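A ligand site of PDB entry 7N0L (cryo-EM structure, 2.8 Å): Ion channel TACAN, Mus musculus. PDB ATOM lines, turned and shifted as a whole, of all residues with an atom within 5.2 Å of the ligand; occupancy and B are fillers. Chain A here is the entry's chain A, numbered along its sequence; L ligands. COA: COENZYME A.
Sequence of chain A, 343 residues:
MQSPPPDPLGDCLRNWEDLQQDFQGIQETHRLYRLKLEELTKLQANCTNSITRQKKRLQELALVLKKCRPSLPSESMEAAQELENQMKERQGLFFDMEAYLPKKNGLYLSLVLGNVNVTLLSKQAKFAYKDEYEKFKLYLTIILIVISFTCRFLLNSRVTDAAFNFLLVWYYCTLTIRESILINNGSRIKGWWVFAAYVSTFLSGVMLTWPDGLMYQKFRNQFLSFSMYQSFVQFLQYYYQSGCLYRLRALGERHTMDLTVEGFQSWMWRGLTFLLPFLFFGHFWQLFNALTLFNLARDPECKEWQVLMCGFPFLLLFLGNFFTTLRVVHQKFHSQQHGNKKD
The backbone carbonyl oxygen (O) of Leu 279 sits close to a ring nitrogen (ND1) of His 283, 3.0 Å away. The side-chain amino group (NZ) of Lys 190 sits close to the side-chain amide nitrogen (NE2) of Gln 331, at 3.4 Å. OG1 of Thr 325 lies within hydrogen-bond range of O of Asn 321. O of Gly 282 lies close to OE1 of Gln 286 (3.4 Å). OH of Tyr 133 lies within hydrogen-bond range of OE2 of Glu 179 (2.8 Å). OH of Tyr 133 is in hydrogen-bond range of NZ of Lys 137 (3.4 Å). OE1 of Gln 286 sits at hydrogen-bond distance from ND2 of Asn 321 (3.5 Å).
OH of Tyr 133 touches C2A of the ligand (3.8 Å). Glu 179 touches the ligand (OE2 to C2A, 3.9 Å). Arg 188 touches the ligand (O to C5B, 3.2 Å). Ile 189 touches the ligand (CG1 to O4B, 3.4 Å). Trp 193 touches the ligand (CZ3 to C6P, 3.4 Å). CZ of Phe 226 touches S1P of the ligand, at 3.5 Å. Leu 272 touches the ligand. CD1 of Leu 275 touches CEP of the ligand, at 3.7 Å. Leu 279 touches the ligand. O of Gly 282 touches S1P of the ligand (3.8 Å). Gln 286 touches the ligand. OG1 of Thr 325 touches OAP of the ligand (3.5 Å). CG1 of Val 328 touches CDP of the ligand, at 3.7 Å. Gln 331 touches the ligand (NE2 to O2A, 3.8 Å). The nearest printed residue that does not touch the ligand is Lys 137 (4.2 Å).
An oxygen (O1A) of the ligand is in salt-bridge range of the side-chain amino group (NZ) of Lys 332 (2.7 Å). The side-chain amino group (NZ) of Lys 130 is in salt-bridge range of an oxygen (O9A) of the ligand. The side-chain hydroxyl (OG) of Ser 187 sits at hydrogen-bond distance from an oxygen (O7A) of the ligand (2.8 Å). N4P of the ligand lies within hydrogen-bond range of NE2 of His 283 (3.0 Å). An oxygen (O5A) of the ligand sits close to the side-chain amide oxygen of Gln 241, at 3.0 Å. An oxygen (O5P) of the ligand sits close to the side-chain amide oxygen (OE1) of Gln 237 (3.1 Å). An oxygen (O4A) of the ligand sits at hydrogen-bond distance from the side-chain hydroxyl (OH) of Tyr 240. O2A of the ligand lies within salt-bridge range of NZ of Lys 190, at 3.4 Å. NE2 of Gln 230 lies close to S1P of the ligand.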
ATOM      1  N   LYS A 130       0.956  27.601  -7.175  1.00  0.00           N
ATOM      2  CA  LYS A 130       0.711  27.409  -8.597  1.00  0.00           C
ATOM      3  C   LYS A 130       1.575  28.318  -9.448  1.00  0.00           C
ATOM      4  O   LYS A 130       1.771  28.030 -10.637  1.00  0.00           O
ATOM      5  CB  LYS A 130      -0.758  27.641  -8.929  1.00  0.00           C
ATOM      6  CG  LYS A 130      -1.206  26.849 -10.140  1.00  0.00           C
ATOM      7  CD  LYS A 130      -2.365  27.522 -10.861  1.00  0.00           C
ATOM      8  CE  LYS A 130      -2.558  26.916 -12.242  1.00  0.00           C
ATOM      9  NZ  LYS A 130      -3.385  27.784 -13.118  1.00  0.00           N
ATOM     10  N   TYR A 133       4.781  26.469  -9.521  1.00  0.00           N
ATOM     11  CA  TYR A 133       4.634  25.300 -10.384  1.00  0.00           C
ATOM     12  C   TYR A 133       4.799  25.660 -11.853  1.00  0.00           C
ATOM     13  O   TYR A 133       5.382  24.880 -12.612  1.00  0.00           O
ATOM     14  CB  TYR A 133       3.269  24.659 -10.147  1.00  0.00           C
ATOM     15  CG  TYR A 133       2.834  23.701 -11.230  1.00  0.00           C
ATOM     16  CD1 TYR A 133       3.400  22.437 -11.320  1.00  0.00           C
ATOM     17  CD2 TYR A 133       1.865  24.050 -12.152  1.00  0.00           C
ATOM     18  CE1 TYR A 133       3.004  21.559 -12.299  1.00  0.00           C
ATOM     19  CE2 TYR A 133       1.466  23.179 -13.137  1.00  0.00           C
ATOM     20  CZ  TYR A 133       2.039  21.936 -13.210  1.00  0.00           C
ATOM     21  OH  TYR A 133       1.652  21.064 -14.187  1.00  0.00           O
ATOM     22  N   LYS A 137       7.972  24.345 -14.402  1.00  0.00           N
ATOM     23  CA  LYS A 137       7.867  23.820 -15.759  1.00  0.00           C
ATOM     24  C   LYS A 137       8.624  24.674 -16.762  1.00  0.00           C
ATOM     25  O   LYS A 137       8.997  24.167 -17.820  1.00  0.00           O
ATOM     26  CB  LYS A 137       6.401  23.713 -16.176  1.00  0.00           C
ATOM     27  CG  LYS A 137       5.543  22.872 -15.260  1.00  0.00           C
ATOM     28  CD  LYS A 137       4.116  22.818 -15.760  1.00  0.00           C
ATOM     29  CE  LYS A 137       4.013  22.048 -17.049  1.00  0.00           C
ATOM     30  NZ  LYS A 137       2.605  21.671 -17.360  1.00  0.00           N
ATOM     31  N   GLU A 179       1.207  18.123  -9.884  1.00  0.00           N
ATOM     32  CA  GLU A 179      -0.178  18.237 -10.342  1.00  0.00           C
ATOM     33  C   GLU A 179      -1.141  17.506  -9.432  1.00  0.00           C
ATOM     34  O   GLU A 179      -2.349  17.751  -9.502  1.00  0.00           O
ATOM     35  CB  GLU A 179      -0.305  17.709 -11.765  1.00  0.00           C
ATOM     36  CG  GLU A 179       0.439  18.531 -12.794  1.00  0.00           C
ATOM     37  CD  GLU A 179       0.550  17.834 -14.141  1.00  0.00           C
ATOM     38  OE1 GLU A 179       0.323  16.606 -14.196  1.00  0.00           O
ATOM     39  OE2 GLU A 179       0.866  18.514 -15.140  1.00  0.00           O
ATOM     40  N   GLY A 186      -7.561  22.527  -4.751  1.00  0.00           N
ATOM     41  CA  GLY A 186      -8.551  23.340  -5.441  1.00  0.00           C
ATOM     42  C   GLY A 186      -8.388  23.539  -6.933  1.00  0.00           C
ATOM     43  O   GLY A 186      -9.051  24.423  -7.485  1.00  0.00           O
ATOM     44  N   SER A 187      -7.559  22.746  -7.613  1.00  0.00           N
ATOM     45  CA  SER A 187      -7.327  22.953  -9.040  1.00  0.00           C
ATOM     46  C   SER A 187      -8.244  22.046  -9.865  1.00  0.00           C
ATOM     47  O   SER A 187      -8.420  20.869  -9.553  1.00  0.00           O
ATOM     48  CB  SER A 187      -5.871  22.675  -9.414  1.00  0.00           C
ATOM     49  OG  SER A 187      -5.134  23.881  -9.468  1.00  0.00           O
ATOM     50  N   ARG A 188      -8.815  22.630 -10.917  1.00  0.00           N
ATOM     51  CA  ARG A 188      -9.722  21.917 -11.821  1.00  0.00           C
ATOM     52  C   ARG A 188      -8.994  21.341 -13.024  1.00  0.00           C
ATOM     53  O   ARG A 188      -9.400  21.556 -14.162  1.00  0.00           O
ATOM     54  CB  ARG A 188     -10.840  22.849 -12.261  1.00  0.00           C
ATOM     55  CG  ARG A 188     -11.311  23.806 -11.187  1.00  0.00           C
ATOM     56  CD  ARG A 188     -12.350  23.162 -10.290  1.00  0.00           C
ATOM     57  NE  ARG A 188     -13.321  24.132  -9.798  1.00  0.00           N
ATOM     58  CZ  ARG A 188     -14.239  23.876  -8.885  1.00  0.00           C
ATOM     59  NH1 ARG A 188     -14.314  22.654  -8.354  1.00  0.00           N
ATOM     60  NH2 ARG A 188     -15.079  24.818  -8.498  1.00  0.00           N
ATOM     61  N   ILE A 189      -7.917  20.602 -12.789  1.00  0.00           N
ATOM     62  CA  ILE A 189      -7.154  20.018 -13.882  1.00  0.00           C
ATOM     63  C   ILE A 189      -7.931  18.845 -14.456  1.00  0.00           C
ATOM     64  O   ILE A 189      -8.252  17.888 -13.743  1.00  0.00           O
ATOM     65  CB  ILE A 189      -5.761  19.590 -13.427  1.00  0.00           C
ATOM     66  CG1 ILE A 189      -5.108  20.707 -12.613  1.00  0.00           C
ATOM     67  CG2 ILE A 189      -4.884  19.226 -14.608  1.00  0.00           C
ATOM     68  CD1 ILE A 189      -3.747  20.347 -12.076  1.00  0.00           C
ATOM     69  N   LYS A 190      -8.240  18.911 -15.758  1.00  0.00           N
ATOM     70  CA  LYS A 190      -8.985  17.837 -16.398  1.00  0.00           C
ATOM     71  C   LYS A 190      -8.214  16.520 -16.294  1.00  0.00           C
ATOM     72  O   LYS A 190      -6.986  16.500 -16.263  1.00  0.00           O
ATOM     73  CB  LYS A 190      -9.256  18.169 -17.868  1.00  0.00           C
ATOM     74  CG  LYS A 190     -10.268  19.284 -18.058  1.00  0.00           C
ATOM     75  CD  LYS A 190     -10.407  19.667 -19.510  1.00  0.00           C
ATOM     76  CE  LYS A 190     -11.726  20.378 -19.764  1.00  0.00           C
ATOM     77  NZ  LYS A 190     -12.074  21.303 -18.660  1.00  0.00           N
ATOM     78  N   TRP A 193      -4.945  15.668 -18.594  1.00  0.00           N
ATOM     79  CA  TRP A 193      -3.649  16.317 -18.438  1.00  0.00           C
ATOM     80  C   TRP A 193      -2.796  15.660 -17.366  1.00  0.00           C
ATOM     81  O   TRP A 193      -1.567  15.654 -17.469  1.00  0.00           O
ATOM     82  CB  TRP A 193      -3.837  17.797 -18.132  1.00  0.00           C
ATOM     83  CG  TRP A 193      -4.712  18.520 -19.099  1.00  0.00           C
ATOM     84  CD1 TRP A 193      -5.798  19.291 -18.811  1.00  0.00           C
ATOM     85  CD2 TRP A 193      -4.581  18.545 -20.526  1.00  0.00           C
ATOM     86  NE1 TRP A 193      -6.349  19.791 -19.955  1.00  0.00           N
ATOM     87  CE2 TRP A 193      -5.618  19.346 -21.030  1.00  0.00           C
ATOM     88  CE3 TRP A 193      -3.686  17.970 -21.435  1.00  0.00           C
ATOM     89  CZ2 TRP A 193      -5.789  19.586 -22.386  1.00  0.00           C
ATOM     90  CZ3 TRP A 193      -3.859  18.209 -22.776  1.00  0.00           C
ATOM     91  CH2 TRP A 193      -4.892  19.011 -23.236  1.00  0.00           C
ATOM     92  N   PHE A 226      10.996  16.550 -31.816  1.00  0.00           N
ATOM     93  CA  PHE A 226       9.645  16.798 -31.314  1.00  0.00           C
ATOM     94  C   PHE A 226       9.691  17.280 -29.867  1.00  0.00           C
ATOM     95  O   PHE A 226       9.077  18.293 -29.530  1.00  0.00           O
ATOM     96  CB  PHE A 226       8.805  15.531 -31.419  1.00  0.00           C
ATOM     97  CG  PHE A 226       7.528  15.588 -30.622  1.00  0.00           C
ATOM     98  CD1 PHE A 226       7.400  14.869 -29.452  1.00  0.00           C
ATOM     99  CD2 PHE A 226       6.475  16.375 -31.043  1.00  0.00           C
ATOM    100  CE1 PHE A 226       6.240  14.928 -28.722  1.00  0.00           C
ATOM    101  CE2 PHE A 226       5.307  16.428 -30.315  1.00  0.00           C
ATOM    102  CZ  PHE A 226       5.196  15.705 -29.157  1.00  0.00           C
ATOM    103  N   TYR A 229      10.514  20.675 -29.874  1.00  0.00           N
ATOM    104  CA  TYR A 229       9.353  21.506 -30.172  1.00  0.00           C
ATOM    105  C   TYR A 229       8.398  21.543 -28.996  1.00  0.00           C
ATOM    106  O   TYR A 229       7.879  22.607 -28.637  1.00  0.00           O
ATOM    107  CB  TYR A 229       8.652  20.990 -31.421  1.00  0.00           C
ATOM    108  CG  TYR A 229       7.305  21.616 -31.687  1.00  0.00           C
ATOM    109  CD1 TYR A 229       6.138  21.009 -31.255  1.00  0.00           C
ATOM    110  CD2 TYR A 229       7.193  22.800 -32.390  1.00  0.00           C
ATOM    111  CE1 TYR A 229       4.905  21.582 -31.494  1.00  0.00           C
ATOM    112  CE2 TYR A 229       5.970  23.379 -32.641  1.00  0.00           C
ATOM    113  CZ  TYR A 229       4.829  22.763 -32.186  1.00  0.00           C
ATOM    114  OH  TYR A 229       3.600  23.330 -32.432  1.00  0.00           O
ATOM    115  N   GLN A 230       8.150  20.383 -28.383  1.00  0.00           N
ATOM    116  CA  GLN A 230       7.262  20.321 -27.232  1.00  0.00           C
ATOM    117  C   GLN A 230       7.750  21.175 -26.069  1.00  0.00           C
ATOM    118  O   GLN A 230       6.952  21.553 -25.207  1.00  0.00           O
ATOM    119  CB  GLN A 230       7.102  18.872 -26.769  1.00  0.00           C
ATOM    120  CG  GLN A 230       5.916  18.645 -25.864  1.00  0.00           C
ATOM    121  CD  GLN A 230       5.687  17.175 -25.552  1.00  0.00           C
ATOM    122  OE1 GLN A 230       6.635  16.392 -25.462  1.00  0.00           O
ATOM    123  NE2 GLN A 230       4.425  16.804 -25.391  1.00  0.00           N
ATOM    124  N   VAL A 233       6.752  24.945 -27.227  1.00  0.00           N
ATOM    125  CA  VAL A 233       5.342  25.242 -26.990  1.00  0.00           C
ATOM    126  C   VAL A 233       5.050  25.397 -25.502  1.00  0.00           C
ATOM    127  O   VAL A 233       4.043  26.004 -25.130  1.00  0.00           O
ATOM    128  CB  VAL A 233       4.457  24.162 -27.629  1.00  0.00           C
ATOM    129  CG1 VAL A 233       4.489  22.888 -26.815  1.00  0.00           C
ATOM    130  CG2 VAL A 233       3.032  24.658 -27.780  1.00  0.00           C
ATOM    131  N   GLN A 237       2.886  28.136 -23.466  1.00  0.00           N
ATOM    132  CA  GLN A 237       1.965  27.721 -22.426  1.00  0.00           C
ATOM    133  C   GLN A 237       2.251  28.465 -21.129  1.00  0.00           C
ATOM    134  O   GLN A 237       1.314  28.878 -20.435  1.00  0.00           O
ATOM    135  CB  GLN A 237       2.057  26.216 -22.194  1.00  0.00           C
ATOM    136  CG  GLN A 237       1.285  25.392 -23.196  1.00  0.00           C
ATOM    137  CD  GLN A 237       1.578  23.919 -23.070  1.00  0.00           C
ATOM    138  OE1 GLN A 237       1.903  23.260 -24.049  1.00  0.00           O
ATOM    139  NE2 GLN A 237       1.473  23.399 -21.862  1.00  0.00           N
ATOM    140  N   TYR A 240       0.993  32.113 -21.311  1.00  0.00           N
ATOM    141  CA  TYR A 240      -0.467  32.115 -21.238  1.00  0.00           C
ATOM    142  C   TYR A 240      -0.948  31.657 -19.867  1.00  0.00           C
ATOM    143  O   TYR A 240      -1.799  32.314 -19.253  1.00  0.00           O
ATOM    144  CB  TYR A 240      -1.053  31.229 -22.342  1.00  0.00           C
ATOM    145  CG  TYR A 240      -2.478  30.785 -22.133  1.00  0.00           C
ATOM    146  CD1 TYR A 240      -2.776  29.585 -21.493  1.00  0.00           C
ATOM    147  CD2 TYR A 240      -3.537  31.555 -22.599  1.00  0.00           C
ATOM    148  CE1 TYR A 240      -4.079  29.178 -21.304  1.00  0.00           C
ATOM    149  CE2 TYR A 240      -4.840  31.148 -22.410  1.00  0.00           C
ATOM    150  CZ  TYR A 240      -5.100  29.964 -21.771  1.00  0.00           C
ATOM    151  OH  TYR A 240      -6.403  29.557 -21.582  1.00  0.00           O
ATOM    152  N   GLN A 241      -0.412  30.535 -19.374  1.00  0.00           N
ATOM    153  CA  GLN A 241      -0.873  29.994 -18.096  1.00  0.00           C
ATOM    154  C   GLN A 241      -0.577  30.952 -16.962  1.00  0.00           C
ATOM    155  O   GLN A 241      -1.408  31.148 -16.072  1.00  0.00           O
ATOM    156  CB  GLN A 241      -0.212  28.643 -17.843  1.00  0.00           C
ATOM    157  CG  GLN A 241      -1.153  27.580 -17.315  1.00  0.00           C
ATOM    158  CD  GLN A 241      -1.818  26.805 -18.437  1.00  0.00           C
ATOM    159  OE1 GLN A 241      -2.696  27.328 -19.125  1.00  0.00           O
ATOM    160  NE2 GLN A 241      -1.392  25.565 -18.645  1.00  0.00           N
ATOM    161  N   LEU A 272      -5.150  32.153 -26.350  1.00  0.00           N
ATOM    162  CA  LEU A 272      -5.600  30.869 -26.875  1.00  0.00           C
ATOM    163  C   LEU A 272      -5.509  30.830 -28.392  1.00  0.00           C
ATOM    164  O   LEU A 272      -5.128  29.811 -28.967  1.00  0.00           O
ATOM    165  CB  LEU A 272      -7.031  30.596 -26.420  1.00  0.00           C
ATOM    166  CG  LEU A 272      -7.249  29.612 -25.279  1.00  0.00           C
ATOM    167  CD1 LEU A 272      -8.668  29.057 -25.345  1.00  0.00           C
ATOM    168  CD2 LEU A 272      -6.238  28.489 -25.347  1.00  0.00           C
ATOM    169  N   LEU A 275      -2.149  30.096 -29.285  1.00  0.00           N
ATOM    170  CA  LEU A 275      -1.676  28.846 -28.711  1.00  0.00           C
ATOM    171  C   LEU A 275      -2.178  27.622 -29.450  1.00  0.00           C
ATOM    172  O   LEU A 275      -1.431  26.653 -29.599  1.00  0.00           O
ATOM    173  CB  LEU A 275      -2.083  28.735 -27.241  1.00  0.00           C
ATOM    174  CG  LEU A 275      -0.991  28.610 -26.184  1.00  0.00           C
ATOM    175  CD1 LEU A 275      -1.591  28.255 -24.850  1.00  0.00           C
ATOM    176  CD2 LEU A 275       0.042  27.575 -26.590  1.00  0.00           C
ATOM    177  N   LEU A 276      -3.419  27.644 -29.917  1.00  0.00           N
ATOM    178  CA  LEU A 276      -3.994  26.478 -30.579  1.00  0.00           C
ATOM    179  C   LEU A 276      -3.203  26.036 -31.812  1.00  0.00           C
ATOM    180  O   LEU A 276      -2.962  24.825 -31.949  1.00  0.00           O
ATOM    181  CB  LEU A 276      -5.457  26.764 -30.934  1.00  0.00           C
ATOM    182  CG  LEU A 276      -6.398  26.944 -29.742  1.00  0.00           C
ATOM    183  CD1 LEU A 276      -7.847  26.891 -30.187  1.00  0.00           C
ATOM    184  CD2 LEU A 276      -6.128  25.906 -28.673  1.00  0.00           C
ATOM    185  N   PHE A 278      -0.089  26.164 -32.347  1.00  0.00           N
ATOM    186  CA  PHE A 278       1.101  25.494 -31.830  1.00  0.00           C
ATOM    187  C   PHE A 278       0.756  24.263 -31.005  1.00  0.00           C
ATOM    188  O   PHE A 278       1.650  23.448 -30.745  1.00  0.00           O
ATOM    189  CB  PHE A 278       1.935  26.473 -30.999  1.00  0.00           C
ATOM    190  CG  PHE A 278       2.400  27.669 -31.766  1.00  0.00           C
ATOM    191  CD1 PHE A 278       3.684  27.715 -32.273  1.00  0.00           C
ATOM    192  CD2 PHE A 278       1.560  28.744 -31.972  1.00  0.00           C
ATOM    193  CE1 PHE A 278       4.126  28.817 -32.973  1.00  0.00           C
ATOM    194  CE2 PHE A 278       1.990  29.847 -32.681  1.00  0.00           C
ATOM    195  CZ  PHE A 278       3.278  29.887 -33.181  1.00  0.00           C
ATOM    196  N   LEU A 279      -0.493  24.125 -30.575  1.00  0.00           N
ATOM    197  CA  LEU A 279      -0.910  22.898 -29.907  1.00  0.00           C
ATOM    198  C   LEU A 279      -1.310  21.825 -30.913  1.00  0.00           C
ATOM    199  O   LEU A 279      -1.051  20.645 -30.688  1.00  0.00           O
ATOM    200  CB  LEU A 279      -2.071  23.165 -28.956  1.00  0.00           C
ATOM    201  CG  LEU A 279      -1.796  23.953 -27.684  1.00  0.00           C
ATOM    202  CD1 LEU A 279      -3.091  24.142 -26.926  1.00  0.00           C
ATOM    203  CD2 LEU A 279      -0.766  23.242 -26.836  1.00  0.00           C
ATOM    204  N   GLY A 282       1.511  20.293 -32.654  1.00  0.00           N
ATOM    205  CA  GLY A 282       2.144  19.351 -31.762  1.00  0.00           C
ATOM    206  C   GLY A 282       1.344  18.076 -31.642  1.00  0.00           C
ATOM    207  O   GLY A 282       1.908  16.994 -31.478  1.00  0.00           O
ATOM    208  N   HIS A 283       0.017  18.186 -31.702  1.00  0.00           N
ATOM    209  CA  HIS A 283      -0.819  17.000 -31.641  1.00  0.00           C
ATOM    210  C   HIS A 283      -0.729  16.186 -32.916  1.00  0.00           C
ATOM    211  O   HIS A 283      -0.862  14.956 -32.884  1.00  0.00           O
ATOM    212  CB  HIS A 283      -2.277  17.382 -31.371  1.00  0.00           C
ATOM    213  CG  HIS A 283      -2.473  18.137 -30.091  1.00  0.00           C
ATOM    214  ND1 HIS A 283      -3.479  19.056 -29.915  1.00  0.00           N
ATOM    215  CD2 HIS A 283      -1.789  18.099 -28.922  1.00  0.00           C
ATOM    216  CE1 HIS A 283      -3.416  19.551 -28.701  1.00  0.00           C
ATOM    217  NE2 HIS A 283      -2.395  18.987 -28.075  1.00  0.00           N
ATOM    218  N   GLN A 286       2.631  14.227 -32.843  1.00  0.00           N
ATOM    219  CA  GLN A 286       2.499  12.986 -32.112  1.00  0.00           C
ATOM    220  C   GLN A 286       1.806  11.921 -32.960  1.00  0.00           C
ATOM    221  O   GLN A 286       2.166  10.737 -32.904  1.00  0.00           O
ATOM    222  CB  GLN A 286       1.731  13.205 -30.814  1.00  0.00           C
ATOM    223  CG  GLN A 286       2.602  13.505 -29.620  1.00  0.00           C
ATOM    224  CD  GLN A 286       1.913  14.392 -28.617  1.00  0.00           C
ATOM    225  OE1 GLN A 286       0.925  15.049 -28.931  1.00  0.00           O
ATOM    226  NE2 GLN A 286       2.418  14.414 -27.395  1.00  0.00           N
ATOM    227  N   ASN A 321      -4.680  14.266 -26.168  1.00  0.00           N
ATOM    228  CA  ASN A 321      -4.421  15.701 -26.160  1.00  0.00           C
ATOM    229  C   ASN A 321      -5.345  16.426 -27.131  1.00  0.00           C
ATOM    230  O   ASN A 321      -5.942  17.449 -26.791  1.00  0.00           O
ATOM    231  CB  ASN A 321      -2.966  15.985 -26.511  1.00  0.00           C
ATOM    232  CG  ASN A 321      -2.004  15.433 -25.490  1.00  0.00           C
ATOM    233  OD1 ASN A 321      -2.368  15.187 -24.350  1.00  0.00           O
ATOM    234  ND2 ASN A 321      -0.762  15.238 -25.904  1.00  0.00           N
ATOM    235  N   THR A 325      -8.025  19.257 -25.963  1.00  0.00           N
ATOM    236  CA  THR A 325      -7.889  20.662 -26.327  1.00  0.00           C
ATOM    237  C   THR A 325      -9.103  21.151 -27.101  1.00  0.00           C
ATOM    238  O   THR A 325      -9.502  22.309 -26.956  1.00  0.00           O
ATOM    239  CB  THR A 325      -6.613  20.858 -27.154  1.00  0.00           C
ATOM    240  OG1 THR A 325      -5.487  20.464 -26.365  1.00  0.00           O
ATOM    241  CG2 THR A 325      -6.451  22.307 -27.561  1.00  0.00           C
ATOM    242  N   VAL A 328     -11.676  21.683 -24.374  1.00  0.00           N
ATOM    243  CA  VAL A 328     -11.438  22.932 -23.651  1.00  0.00           C
ATOM    244  C   VAL A 328     -11.930  24.120 -24.455  1.00  0.00           C
ATOM    245  O   VAL A 328     -12.485  25.079 -23.903  1.00  0.00           O
ATOM    246  CB  VAL A 328      -9.937  23.057 -23.293  1.00  0.00           C
ATOM    247  CG1 VAL A 328      -9.636  24.437 -22.736  1.00  0.00           C
ATOM    248  CG2 VAL A 328      -9.550  22.003 -22.293  1.00  0.00           C
ATOM    249  N   GLN A 331     -15.859  24.240 -24.437  1.00  0.00           N
ATOM    250  CA  GLN A 331     -16.471  24.807 -23.252  1.00  0.00           C
ATOM    251  C   GLN A 331     -16.219  26.300 -23.124  1.00  0.00           C
ATOM    252  O   GLN A 331     -17.064  27.021 -22.581  1.00  0.00           O
ATOM    253  CB  GLN A 331     -15.988  24.082 -21.987  1.00  0.00           C
ATOM    254  CG  GLN A 331     -14.537  24.342 -21.634  1.00  0.00           C
ATOM    255  CD  GLN A 331     -14.292  24.388 -20.149  1.00  0.00           C
ATOM    256  OE1 GLN A 331     -15.237  24.489 -19.359  1.00  0.00           O
ATOM    257  NE2 GLN A 331     -13.030  24.332 -19.755  1.00  0.00           N
ATOM    258  N   LYS A 332     -15.073  26.786 -23.620  1.00  0.00           N
ATOM    259  CA  LYS A 332     -14.807  28.225 -23.596  1.00  0.00           C
ATOM    260  C   LYS A 332     -15.577  28.961 -24.673  1.00  0.00           C
ATOM    261  O   LYS A 332     -15.814  30.164 -24.529  1.00  0.00           O
ATOM    262  CB  LYS A 332     -13.313  28.476 -23.761  1.00  0.00           C
ATOM    263  CG  LYS A 332     -12.467  27.963 -22.618  1.00  0.00           C
ATOM    264  CD  LYS A 332     -11.122  28.639 -22.576  1.00  0.00           C
ATOM    265  CE  LYS A 332     -10.178  27.912 -21.645  1.00  0.00           C
ATOM    266  NZ  LYS A 332     -10.893  27.362 -20.464  1.00  0.00           N
HETATM  267  N1A COA L   1      -1.514  20.866 -17.263  1.00  0.00           N
HETATM  268  C2A COA L   1      -1.689  21.300 -16.042  1.00  0.00           C
HETATM  269  N3A COA L   1      -2.705  22.209 -15.768  1.00  0.00           N
HETATM  270  C4A COA L   1      -3.488  22.638 -16.743  1.00  0.00           C
HETATM  271  C5A COA L   1      -3.319  22.201 -17.993  1.00  0.00           C
HETATM  272  C6A COA L   1      -2.320  21.297 -18.253  1.00  0.00           C
HETATM  273  N6A COA L   1      -1.842  20.611 -19.477  1.00  0.00           N
HETATM  274  N7A COA L   1      -4.231  22.782 -18.771  1.00  0.00           N
HETATM  275  C8A COA L   1      -4.969  23.581 -18.010  1.00  0.00           C
HETATM  276  N9A COA L   1      -4.505  23.491 -16.760  1.00  0.00           N
HETATM  277  C1B COA L   1      -4.865  24.090 -15.484  1.00  0.00           C
HETATM  278  C2B COA L   1      -5.359  25.327 -15.661  1.00  0.00           C
HETATM  279  O2B COA L   1      -4.334  26.325 -15.345  1.00  0.00           O
HETATM  280  C3B COA L   1      -6.505  25.409 -14.664  1.00  0.00           C
HETATM  281  O3B COA L   1      -5.985  25.633 -13.441  1.00  0.00           O
HETATM  282  P3B COA L   1      -6.874  26.419 -12.282  1.00  0.00           P
HETATM  283  O7A COA L   1      -6.760  25.656 -10.957  1.00  0.00           O
HETATM  284  O8A COA L   1      -8.322  26.492 -12.707  1.00  0.00           O
HETATM  285  O9A COA L   1      -6.326  27.822 -12.084  1.00  0.00           O
HETATM  286  C4B COA L   1      -7.102  23.952 -14.714  1.00  0.00           C
HETATM  287  O4B COA L   1      -6.031  23.204 -14.781  1.00  0.00           O
HETATM  288  C5B COA L   1      -7.953  23.725 -15.948  1.00  0.00           C
HETATM  289  O5B COA L   1      -8.351  24.941 -16.561  1.00  0.00           O
HETATM  290  P1A COA L   1      -8.853  24.862 -18.168  1.00  0.00           P
HETATM  291  O1A COA L   1      -9.827  25.981 -18.461  1.00  0.00           O
HETATM  292  O2A COA L   1      -9.549  23.550 -18.399  1.00  0.00           O
HETATM  293  O3A COA L   1      -7.567  24.954 -19.162  1.00  0.00           O
HETATM  294  P2A COA L   1      -6.849  26.343 -19.664  1.00  0.00           P
HETATM  295  O4A COA L   1      -7.826  27.520 -19.573  1.00  0.00           O
HETATM  296  O5A COA L   1      -5.633  26.633 -18.788  1.00  0.00           O
HETATM  297  O6A COA L   1      -6.340  26.154 -21.255  1.00  0.00           O
HETATM  298  CBP COA L   1      -4.894  24.952 -22.817  1.00  0.00           C
HETATM  299  CCP COA L   1      -4.997  25.638 -21.471  1.00  0.00           C
HETATM  300  CDP COA L   1      -6.161  25.258 -23.644  1.00  0.00           C
HETATM  301  CEP COA L   1      -3.659  25.481 -23.579  1.00  0.00           C
HETATM  302  CAP COA L   1      -4.803  23.456 -22.606  1.00  0.00           C
HETATM  303  OAP COA L   1      -5.413  22.815 -23.709  1.00  0.00           O
HETATM  304  C9P COA L   1      -3.365  22.952 -22.497  1.00  0.00           C
HETATM  305  O9P COA L   1      -2.656  23.330 -21.640  1.00  0.00           O
HETATM  306  N8P COA L   1      -2.868  21.983 -23.463  1.00  0.00           N
HETATM  307  C7P COA L   1      -1.468  21.481 -23.351  1.00  0.00           C
HETATM  308  C6P COA L   1      -1.359  20.150 -24.049  1.00  0.00           C
HETATM  309  C5P COA L   1      -0.058  20.129 -24.911  1.00  0.00           C
HETATM  310  O5P COA L   1       0.981  20.364 -24.422  1.00  0.00           O
HETATM  311  N4P COA L   1      -0.134  19.803 -26.337  1.00  0.00           N
HETATM  312  C3P COA L   1       1.098  19.786 -27.162  1.00  0.00           C
HETATM  313  C2P COA L   1       1.775  18.435 -27.079  1.00  0.00           C
HETATM  314  S1P COA L   1       3.189  18.429 -28.185  1.00  0.00           S
